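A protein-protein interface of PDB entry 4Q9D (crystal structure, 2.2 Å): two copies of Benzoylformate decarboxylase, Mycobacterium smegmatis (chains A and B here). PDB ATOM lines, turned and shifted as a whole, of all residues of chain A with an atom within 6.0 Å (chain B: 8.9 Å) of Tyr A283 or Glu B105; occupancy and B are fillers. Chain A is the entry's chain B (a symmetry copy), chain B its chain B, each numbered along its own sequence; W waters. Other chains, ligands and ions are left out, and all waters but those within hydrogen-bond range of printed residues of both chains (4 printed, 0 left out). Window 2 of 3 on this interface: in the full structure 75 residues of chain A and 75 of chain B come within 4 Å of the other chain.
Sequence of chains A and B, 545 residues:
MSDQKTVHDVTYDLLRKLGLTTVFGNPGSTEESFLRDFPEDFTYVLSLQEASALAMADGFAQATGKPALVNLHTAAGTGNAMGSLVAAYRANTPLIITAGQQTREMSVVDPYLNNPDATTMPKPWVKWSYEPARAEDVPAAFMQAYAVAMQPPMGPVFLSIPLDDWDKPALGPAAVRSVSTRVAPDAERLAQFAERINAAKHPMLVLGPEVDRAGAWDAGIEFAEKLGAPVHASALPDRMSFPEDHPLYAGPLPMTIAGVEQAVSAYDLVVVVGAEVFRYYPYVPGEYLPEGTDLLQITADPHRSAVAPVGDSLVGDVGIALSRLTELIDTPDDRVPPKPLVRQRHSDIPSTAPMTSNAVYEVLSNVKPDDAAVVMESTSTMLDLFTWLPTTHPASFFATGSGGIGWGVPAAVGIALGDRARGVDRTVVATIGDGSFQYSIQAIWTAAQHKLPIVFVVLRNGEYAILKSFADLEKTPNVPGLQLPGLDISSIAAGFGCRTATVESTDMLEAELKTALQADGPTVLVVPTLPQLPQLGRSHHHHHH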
ATOM      1  N   THR A 256       2.952  -7.503 -19.227  1.00  0.00           N
ATOM      2  CA  THR A 256       1.968  -6.415 -19.221  1.00  0.00           C
ATOM      3  C   THR A 256       1.713  -5.915 -20.646  1.00  0.00           C
ATOM      4  O   THR A 256       2.524  -6.134 -21.557  1.00  0.00           O
ATOM      5  CB  THR A 256       2.444  -5.204 -18.401  1.00  0.00           C
ATOM      6  OG1 THR A 256       3.557  -4.609 -19.084  1.00  0.00           O
ATOM      7  CG2 THR A 256       2.881  -5.623 -16.992  1.00  0.00           C
ATOM      8  N   ILE A 257       0.596  -5.226 -20.830  1.00  0.00           N
ATOM      9  CA  ILE A 257       0.275  -4.620 -22.122  1.00  0.00           C
ATOM     10  C   ILE A 257       1.367  -3.607 -22.538  1.00  0.00           C
ATOM     11  O   ILE A 257       1.936  -3.710 -23.632  1.00  0.00           O
ATOM     12  CB  ILE A 257      -1.117  -3.946 -22.094  1.00  0.00           C
ATOM     13  CG1 ILE A 257      -2.238  -4.985 -21.868  1.00  0.00           C
ATOM     14  CG2 ILE A 257      -1.382  -3.195 -23.414  1.00  0.00           C
ATOM     15  CD1 ILE A 257      -3.570  -4.339 -21.469  1.00  0.00           C
ATOM     16  N   TYR A 281      -0.549 -10.459 -17.052  1.00  0.00           N
ATOM     17  CA  TYR A 281      -0.809 -10.655 -15.630  1.00  0.00           C
ATOM     18  C   TYR A 281      -1.224  -9.332 -14.990  1.00  0.00           C
ATOM     19  O   TYR A 281      -2.402  -8.976 -15.020  1.00  0.00           O
ATOM     20  CB  TYR A 281       0.428 -11.217 -14.928  1.00  0.00           C
ATOM     21  CG  TYR A 281       0.144 -11.815 -13.567  1.00  0.00           C
ATOM     22  CD1 TYR A 281      -1.145 -11.840 -13.053  1.00  0.00           C
ATOM     23  CD2 TYR A 281       1.168 -12.354 -12.799  1.00  0.00           C
ATOM     24  CE1 TYR A 281      -1.408 -12.385 -11.810  1.00  0.00           C
ATOM     25  CE2 TYR A 281       0.914 -12.901 -11.556  1.00  0.00           C
ATOM     26  CZ  TYR A 281      -0.375 -12.914 -11.067  1.00  0.00           C
ATOM     27  OH  TYR A 281      -0.632 -13.459  -9.829  1.00  0.00           O
ATOM     28  N   PRO A 282      -0.271  -8.594 -14.419  1.00  0.00           N
ATOM     29  CA  PRO A 282      -0.620  -7.269 -13.872  1.00  0.00           C
ATOM     30  C   PRO A 282      -1.018  -6.295 -14.974  1.00  0.00           C
ATOM     31  O   PRO A 282      -0.648  -6.478 -16.146  1.00  0.00           O
ATOM     32  CB  PRO A 282       0.671  -6.795 -13.203  1.00  0.00           C
ATOM     33  CG  PRO A 282       1.788  -7.572 -13.886  1.00  0.00           C
ATOM     34  CD  PRO A 282       1.189  -8.835 -14.451  1.00  0.00           C
ATOM     35  N   TYR A 283      -1.807  -5.291 -14.605  1.00  0.00           N
ATOM     36  CA  TYR A 283      -2.302  -4.324 -15.571  1.00  0.00           C
ATOM     37  C   TYR A 283      -1.390  -3.094 -15.637  1.00  0.00           C
ATOM     38  O   TYR A 283      -1.270  -2.389 -14.656  1.00  0.00           O
ATOM     39  CB  TYR A 283      -3.708  -3.872 -15.197  1.00  0.00           C
ATOM     40  CG  TYR A 283      -4.256  -2.914 -16.206  1.00  0.00           C
ATOM     41  CD1 TYR A 283      -4.452  -3.326 -17.512  1.00  0.00           C
ATOM     42  CD2 TYR A 283      -4.555  -1.584 -15.869  1.00  0.00           C
ATOM     43  CE1 TYR A 283      -4.963  -2.473 -18.470  1.00  0.00           C
ATOM     44  CE2 TYR A 283      -5.066  -0.715 -16.826  1.00  0.00           C
ATOM     45  CZ  TYR A 283      -5.266  -1.176 -18.135  1.00  0.00           C
ATOM     46  OH  TYR A 283      -5.755  -0.348 -19.120  1.00  0.00           O
ATOM     47  N   VAL A 284      -0.748  -2.865 -16.784  1.00  0.00           N
ATOM     48  CA  VAL A 284      -0.057  -1.610 -17.054  1.00  0.00           C
ATOM     49  C   VAL A 284      -0.529  -1.176 -18.422  1.00  0.00           C
ATOM     50  O   VAL A 284      -0.272  -1.866 -19.407  1.00  0.00           O
ATOM     51  CB  VAL A 284       1.479  -1.750 -17.051  1.00  0.00           C
ATOM     52  CG1 VAL A 284       2.159  -0.366 -17.347  1.00  0.00           C
ATOM     53  CG2 VAL A 284       1.964  -2.305 -15.698  1.00  0.00           C
ATOM     54  N   PRO A 285      -1.241  -0.036 -18.482  1.00  0.00           N
ATOM     55  CA  PRO A 285      -1.958   0.351 -19.698  1.00  0.00           C
ATOM     56  C   PRO A 285      -1.032   0.668 -20.872  1.00  0.00           C
ATOM     57  O   PRO A 285       0.079   1.175 -20.693  1.00  0.00           O
ATOM     58  CB  PRO A 285      -2.805   1.565 -19.270  1.00  0.00           C
ATOM     59  CG  PRO A 285      -2.194   2.068 -18.011  1.00  0.00           C
ATOM     60  CD  PRO A 285      -1.481   0.891 -17.351  1.00  0.00           C
ATOM     61  N   GLY A 286      -1.509   0.331 -22.066  1.00  0.00           N
ATOM     62  CA  GLY A 286      -0.798   0.579 -23.310  1.00  0.00           C
ATOM     63  C   GLY A 286      -1.676   0.181 -24.491  1.00  0.00           C
ATOM     64  O   GLY A 286      -2.888   0.024 -24.343  1.00  0.00           O
ATOM     65  N   TYR A 288      -2.378  -2.821 -27.171  1.00  0.00           N
ATOM     66  CA  TYR A 288      -2.118  -4.238 -27.393  1.00  0.00           C
ATOM     67  C   TYR A 288      -1.007  -4.408 -28.417  1.00  0.00           C
ATOM     68  O   TYR A 288      -0.069  -5.189 -28.208  1.00  0.00           O
ATOM     69  CB  TYR A 288      -3.397  -4.955 -27.845  1.00  0.00           C
ATOM     70  CG  TYR A 288      -4.410  -5.055 -26.734  1.00  0.00           C
ATOM     71  CD1 TYR A 288      -4.096  -5.742 -25.560  1.00  0.00           C
ATOM     72  CD2 TYR A 288      -5.670  -4.464 -26.838  1.00  0.00           C
ATOM     73  CE1 TYR A 288      -4.998  -5.840 -24.512  1.00  0.00           C
ATOM     74  CE2 TYR A 288      -6.603  -4.565 -25.771  1.00  0.00           C
ATOM     75  CZ  TYR A 288      -6.251  -5.264 -24.626  1.00  0.00           C
ATOM     76  OH  TYR A 288      -7.112  -5.355 -23.550  1.00  0.00           O
ATOM     77  N   GLN B 101     -11.126 -11.097  -9.027  1.00  0.00           N
ATOM     78  CA  GLN B 101     -11.318 -11.370 -10.445  1.00  0.00           C
ATOM     79  C   GLN B 101     -10.363 -10.443 -11.220  1.00  0.00           C
ATOM     80  O   GLN B 101      -9.934  -9.414 -10.687  1.00  0.00           O
ATOM     81  CB  GLN B 101     -12.788 -11.088 -10.777  1.00  0.00           C
ATOM     82  CG  GLN B 101     -13.137 -11.046 -12.258  1.00  0.00           C
ATOM     83  CD  GLN B 101     -12.992 -12.401 -12.944  1.00  0.00           C
ATOM     84  OE1 GLN B 101     -11.878 -12.852 -13.248  1.00  0.00           O
ATOM     85  NE2 GLN B 101     -14.127 -13.023 -13.254  1.00  0.00           N
ATOM     86  N   GLN B 102      -9.994 -10.802 -12.446  1.00  0.00           N
ATOM     87  CA  GLN B 102      -9.141  -9.919 -13.233  1.00  0.00           C
ATOM     88  C   GLN B 102      -9.808  -8.561 -13.476  1.00  0.00           C
ATOM     89  O   GLN B 102     -11.042  -8.435 -13.495  1.00  0.00           O
ATOM     90  CB  GLN B 102      -8.677 -10.577 -14.557  1.00  0.00           C
ATOM     91  CG  GLN B 102      -7.326 -11.294 -14.402  1.00  0.00           C
ATOM     92  CD  GLN B 102      -6.146 -10.288 -14.423  1.00  0.00           C
ATOM     93  OE1 GLN B 102      -6.339  -9.099 -14.180  1.00  0.00           O
ATOM     94  NE2 GLN B 102      -4.941 -10.766 -14.751  1.00  0.00           N
ATOM     95  N   THR B 103      -8.978  -7.539 -13.651  1.00  0.00           N
ATOM     96  CA  THR B 103      -9.460  -6.177 -13.830  1.00  0.00           C
ATOM     97  C   THR B 103     -10.409  -6.082 -15.032  1.00  0.00           C
ATOM     98  O   THR B 103     -10.211  -6.760 -16.053  1.00  0.00           O
ATOM     99  CB  THR B 103      -8.271  -5.164 -14.028  1.00  0.00           C
ATOM    100  OG1 THR B 103      -8.804  -3.953 -14.528  1.00  0.00           O
ATOM    101  CG2 THR B 103      -7.276  -5.684 -15.058  1.00  0.00           C
ATOM    102  N   ARG B 104     -11.439  -5.250 -14.911  1.00  0.00           N
ATOM    103  CA  ARG B 104     -12.313  -4.981 -16.050  1.00  0.00           C
ATOM    104  C   ARG B 104     -11.541  -4.403 -17.242  1.00  0.00           C
ATOM    105  O   ARG B 104     -12.037  -4.444 -18.379  1.00  0.00           O
ATOM    106  CB  ARG B 104     -13.450  -4.020 -15.658  1.00  0.00           C
ATOM    107  CG  ARG B 104     -14.302  -4.495 -14.501  1.00  0.00           C
ATOM    108  CD  ARG B 104     -15.463  -3.544 -14.259  1.00  0.00           C
ATOM    109  NE  ARG B 104     -16.161  -3.890 -13.026  1.00  0.00           N
ATOM    110  CZ  ARG B 104     -17.235  -4.668 -12.943  1.00  0.00           C
ATOM    111  NH1 ARG B 104     -17.768  -5.198 -14.045  1.00  0.00           N
ATOM    112  NH2 ARG B 104     -17.775  -4.909 -11.750  1.00  0.00           N
ATOM    113  N   GLU B 105     -10.331  -3.876 -16.998  1.00  0.00           N
ATOM    114  CA  GLU B 105      -9.544  -3.257 -18.080  1.00  0.00           C
ATOM    115  C   GLU B 105      -8.968  -4.295 -19.039  1.00  0.00           C
ATOM    116  O   GLU B 105      -8.534  -3.943 -20.115  1.00  0.00           O
ATOM    117  CB  GLU B 105      -8.363  -2.431 -17.530  1.00  0.00           C
ATOM    118  CG  GLU B 105      -8.738  -1.448 -16.447  1.00  0.00           C
ATOM    119  CD  GLU B 105      -9.048  -0.085 -17.025  1.00  0.00           C
ATOM    120  OE1 GLU B 105      -9.712   0.716 -16.344  1.00  0.00           O
ATOM    121  OE2 GLU B 105      -8.628   0.177 -18.174  1.00  0.00           O
ATOM    122  N   MET B 106      -8.896  -5.562 -18.633  1.00  0.00           N
ATOM    123  CA  MET B 106      -8.213  -6.580 -19.456  1.00  0.00           C
ATOM    124  C   MET B 106      -8.988  -7.890 -19.585  1.00  0.00           C
ATOM    125  O   MET B 106      -8.605  -8.728 -20.397  1.00  0.00           O
ATOM    126  CB  MET B 106      -6.876  -6.989 -18.816  1.00  0.00           C
ATOM    127  CG  MET B 106      -5.725  -6.145 -19.028  1.00  0.00           C
ATOM    128  SD  MET B 106      -4.185  -7.070 -18.771  1.00  0.00           S
ATOM    129  CE  MET B 106      -4.243  -7.786 -17.122  1.00  0.00           C
ATOM    130  N   SER B 107      -9.997  -8.119 -18.730  1.00  0.00           N
ATOM    131  CA  SER B 107     -10.604  -9.457 -18.620  1.00  0.00           C
ATOM    132  C   SER B 107     -11.159  -9.989 -19.963  1.00  0.00           C
ATOM    133  O   SER B 107     -11.165 -11.193 -20.205  1.00  0.00           O
ATOM    134  CB  SER B 107     -11.651  -9.518 -17.490  1.00  0.00           C
ATOM    135  OG  SER B 107     -12.771  -8.670 -17.741  1.00  0.00           O
ATOM    136  N   VAL B 108     -11.548  -9.092 -20.862  1.00  0.00           N
ATOM    137  CA  VAL B 108     -12.103  -9.515 -22.154  1.00  0.00           C
ATOM    138  C   VAL B 108     -11.141 -10.406 -22.963  1.00  0.00           C
ATOM    139  O   VAL B 108     -11.602 -11.243 -23.724  1.00  0.00           O
ATOM    140  CB  VAL B 108     -12.593  -8.304 -23.022  1.00  0.00           C
ATOM    141  CG1 VAL B 108     -11.414  -7.512 -23.576  1.00  0.00           C
ATOM    142  CG2 VAL B 108     -13.521  -8.789 -24.169  1.00  0.00           C
ATOM    143  N   VAL B 109      -9.822 -10.245 -22.773  1.00  0.00           N
ATOM    144  CA  VAL B 109      -8.844 -11.010 -23.537  1.00  0.00           C
ATOM    145  C   VAL B 109      -8.495 -12.315 -22.805  1.00  0.00           C
ATOM    146  O   VAL B 109      -7.610 -13.056 -23.226  1.00  0.00           O
ATOM    147  CB  VAL B 109      -7.562 -10.176 -23.866  1.00  0.00           C
ATOM    148  CG1 VAL B 109      -7.957  -8.754 -24.423  1.00  0.00           C
ATOM    149  CG2 VAL B 109      -6.641 -10.045 -22.653  1.00  0.00           C
ATOM    150  N   ASP B 110      -9.202 -12.576 -21.710  1.00  0.00           N
ATOM    151  CA  ASP B 110      -8.967 -13.773 -20.891  1.00  0.00           C
ATOM    152  C   ASP B 110      -7.520 -13.866 -20.421  1.00  0.00           C
ATOM    153  O   ASP B 110      -6.814 -14.798 -20.755  1.00  0.00           O
ATOM    154  CB  ASP B 110      -9.426 -15.062 -21.605  1.00  0.00           C
ATOM    155  CG  ASP B 110      -9.464 -16.285 -20.659  1.00  0.00           C
ATOM    156  OD1 ASP B 110      -9.558 -16.099 -19.429  1.00  0.00           O
ATOM    157  OD2 ASP B 110      -9.375 -17.426 -21.136  1.00  0.00           O
ATOM    158  N   PRO B 111      -7.062 -12.862 -19.654  1.00  0.00           N
ATOM    159  CA  PRO B 111      -5.656 -12.819 -19.235  1.00  0.00           C
ATOM    160  C   PRO B 111      -5.334 -13.862 -18.155  1.00  0.00           C
ATOM    161  O   PRO B 111      -6.220 -14.625 -17.740  1.00  0.00           O
ATOM    162  CB  PRO B 111      -5.504 -11.392 -18.685  1.00  0.00           C
ATOM    163  CG  PRO B 111      -6.885 -11.051 -18.133  1.00  0.00           C
ATOM    164  CD  PRO B 111      -7.841 -11.721 -19.140  1.00  0.00           C
ATOM    165  N   TYR B 112      -4.073 -13.906 -17.721  1.00  0.00           N
ATOM    166  CA  TYR B 112      -3.615 -14.894 -16.731  1.00  0.00           C
ATOM    167  C   TYR B 112      -4.427 -14.698 -15.459  1.00  0.00           C
ATOM    168  O   TYR B 112      -4.627 -13.549 -15.020  1.00  0.00           O
ATOM    169  CB  TYR B 112      -2.157 -14.618 -16.388  1.00  0.00           C
ATOM    170  CG  TYR B 112      -1.365 -15.725 -15.714  1.00  0.00           C
ATOM    171  CD1 TYR B 112      -1.083 -16.907 -16.380  1.00  0.00           C
ATOM    172  CD2 TYR B 112      -0.824 -15.541 -14.449  1.00  0.00           C
ATOM    173  CE1 TYR B 112      -0.295 -17.892 -15.805  1.00  0.00           C
ATOM    174  CE2 TYR B 112      -0.044 -16.529 -13.851  1.00  0.00           C
ATOM    175  CZ  TYR B 112       0.219 -17.690 -14.540  1.00  0.00           C
ATOM    176  OH  TYR B 112       1.021 -18.657 -13.985  1.00  0.00           O
ATOM    177  N   PRO B 162     -14.059  -7.904  -9.670  1.00  0.00           N
ATOM    178  CA  PRO B 162     -12.914  -7.417 -10.470  1.00  0.00           C
ATOM    179  C   PRO B 162     -11.986  -6.510  -9.628  1.00  0.00           C
ATOM    180  O   PRO B 162     -12.443  -5.628  -8.905  1.00  0.00           O
ATOM    181  CB  PRO B 162     -13.580  -6.635 -11.602  1.00  0.00           C
ATOM    182  CG  PRO B 162     -14.932  -7.350 -11.796  1.00  0.00           C
ATOM    183  CD  PRO B 162     -15.354  -7.690 -10.342  1.00  0.00           C
ATOM    184  N   LEU B 163     -10.686  -6.759  -9.684  1.00  0.00           N
ATOM    185  CA  LEU B 163      -9.771  -6.121  -8.739  1.00  0.00           C
ATOM    186  C   LEU B 163      -9.736  -4.586  -8.854  1.00  0.00           C
ATOM    187  O   LEU B 163      -9.334  -3.901  -7.917  1.00  0.00           O
ATOM    188  CB  LEU B 163      -8.367  -6.723  -8.879  1.00  0.00           C
ATOM    189  CG  LEU B 163      -7.634  -6.514 -10.220  1.00  0.00           C
ATOM    190  CD1 LEU B 163      -6.831  -5.163 -10.234  1.00  0.00           C
ATOM    191  CD2 LEU B 163      -6.699  -7.672 -10.430  1.00  0.00           C
ATOM    192  N   ASP B 164     -10.183  -4.041  -9.981  1.00  0.00           N
ATOM    193  CA  ASP B 164     -10.082  -2.597 -10.189  1.00  0.00           C
ATOM    194  C   ASP B 164     -11.255  -1.891  -9.560  1.00  0.00           C
ATOM    195  O   ASP B 164     -11.250  -0.672  -9.465  1.00  0.00           O
ATOM    196  CB  ASP B 164      -9.922  -2.228 -11.691  1.00  0.00           C
ATOM    197  CG  ASP B 164     -11.009  -2.840 -12.570  1.00  0.00           C
ATOM    198  OD1 ASP B 164     -11.327  -4.031 -12.384  1.00  0.00           O
ATOM    199  OD2 ASP B 164     -11.546  -2.147 -13.452  1.00  0.00           O
ATOM    200  N   ASP B 165     -12.256  -2.643  -9.106  1.00  0.00           N
ATOM    201  CA  ASP B 165     -13.466  -2.018  -8.581  1.00  0.00           C
ATOM    202  C   ASP B 165     -13.204  -1.232  -7.292  1.00  0.00           C
ATOM    203  O   ASP B 165     -13.844  -0.217  -7.023  1.00  0.00           O
ATOM    204  CB  ASP B 165     -14.591  -3.065  -8.331  1.00  0.00           C
ATOM    205  CG  ASP B 165     -15.288  -3.519  -9.629  1.00  0.00           C
ATOM    206  OD1 ASP B 165     -14.892  -3.056 -10.730  1.00  0.00           O
ATOM    207  OD2 ASP B 165     -16.223  -4.352  -9.555  1.00  0.00           O
ATOM    208  N   LYS B 168     -12.416   2.553  -7.093  1.00  0.00           N
ATOM    209  CA  LYS B 168     -13.315   3.508  -7.724  1.00  0.00           C
ATOM    210  C   LYS B 168     -14.053   4.385  -6.688  1.00  0.00           C
ATOM    211  O   LYS B 168     -14.291   3.961  -5.563  1.00  0.00           O
ATOM    212  CB  LYS B 168     -14.278   2.772  -8.663  1.00  0.00           C
ATOM    213  CG  LYS B 168     -13.531   1.979  -9.765  1.00  0.00           C
ATOM    214  CD  LYS B 168     -12.881   2.979 -10.730  1.00  0.00           C
ATOM    215  CE  LYS B 168     -12.356   2.301 -11.991  1.00  0.00           C
ATOM    216  NZ  LYS B 168     -11.150   1.524 -11.673  1.00  0.00           N
HETATM  217  O   HOH W   1      -1.222  -5.507 -18.584  1.00  0.00           O
HETATM  218  O   HOH W   2      -9.609  -4.573 -22.700  1.00  0.00           O
HETATM  219  O   HOH W   3      -4.251  -7.354 -13.471  1.00  0.00           O
HETATM  220  O   HOH W   4      -6.379   2.397 -18.361  1.00  0.00           O
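Glu B105 touches just these residues of chain A: Tyr A283 (3.1 Å) and Tyr A288 (3.98 Å). Pro A282 touches one residue of chain B. Val A284 touches none of the printed residues of chain B. Of the printed residues of chain A, Gln B102 touches Tyr A281. Of the printed residues of chain B, Ile A257 touches Met B106. Printed residues of chain A within 4 Å of Met B106: Ile A257, Tyr A281, Pro A282 and Tyr A283. Pro B111 touches none of the printed residues of chain A. Arg B104 touches none of the printed residues of chain A. The nearest residue of chain A that does not touch Glu B105 is Ile A257 (5.2 Å). The nearest printed residue of chain B that does not touch Tyr A281 is Pro B111 (5.3 Å).
OG1 of Thr B103 is in hydrogen-bond range of N of Glu B105 (2.9 Å). NE2 of Gln B102 sits at hydrogen-bond distance from O of Tyr B112, 2.8 Å away.
No position is printed for both chains.
Water W1 lies within hydrogen-bond range of O of Pro A282, N of Ile A257, N of Val A284 and SD of Met B106. Water W2 lies within hydrogen-bond range of OH of Tyr A288 (2.8 Å) and O of Glu B105 (2.9 Å). Water W3 lies within hydrogen-bond range of the side-chain amide oxygen of Gln B102, the backbone carbonyl oxygen of Tyr A281 and the backbone NH of Tyr A283. Water W4 bridges the side-chain hydroxyl (OH) of Tyr A283 (2.9 Å) and the side-chain carboxylate (OE2) of Glu B105 (3.2 Å).
Hydrophobic or aromatic side chains of chain A that line the printed part of chain B: Ile A257, Tyr A281, Tyr A283 and Tyr A288. Printed residues of chain B that touch a printed residue of chain A: Gln B102, Glu B105, Met B106, Val B109 and Tyr B112. Hydrophobic or aromatic side chains of chain B that line the printed part of chain A: Met B106, Val B109 and Tyr B112.
The side-chain carboxylate (OE2) of Glu B105 lies within hydrogen-bond range of the side-chain hydroxyl (OH) of Tyr A283, 3.1 Å away. The backbone carbonyl oxygen of Tyr A281 lies within hydrogen-bond range of the side-chain amide nitrogen of Gln B102 (3.1 Å).
Among the printed residues, merely in contact across the chains: Ile A257 with Met B106, Tyr A281 with Met B106, Tyr A281 with Tyr B112, Pro A282 with Met B106, Tyr A283 with Met B106, Tyr A288 with Glu B105 and Tyr A288 with Val B109.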
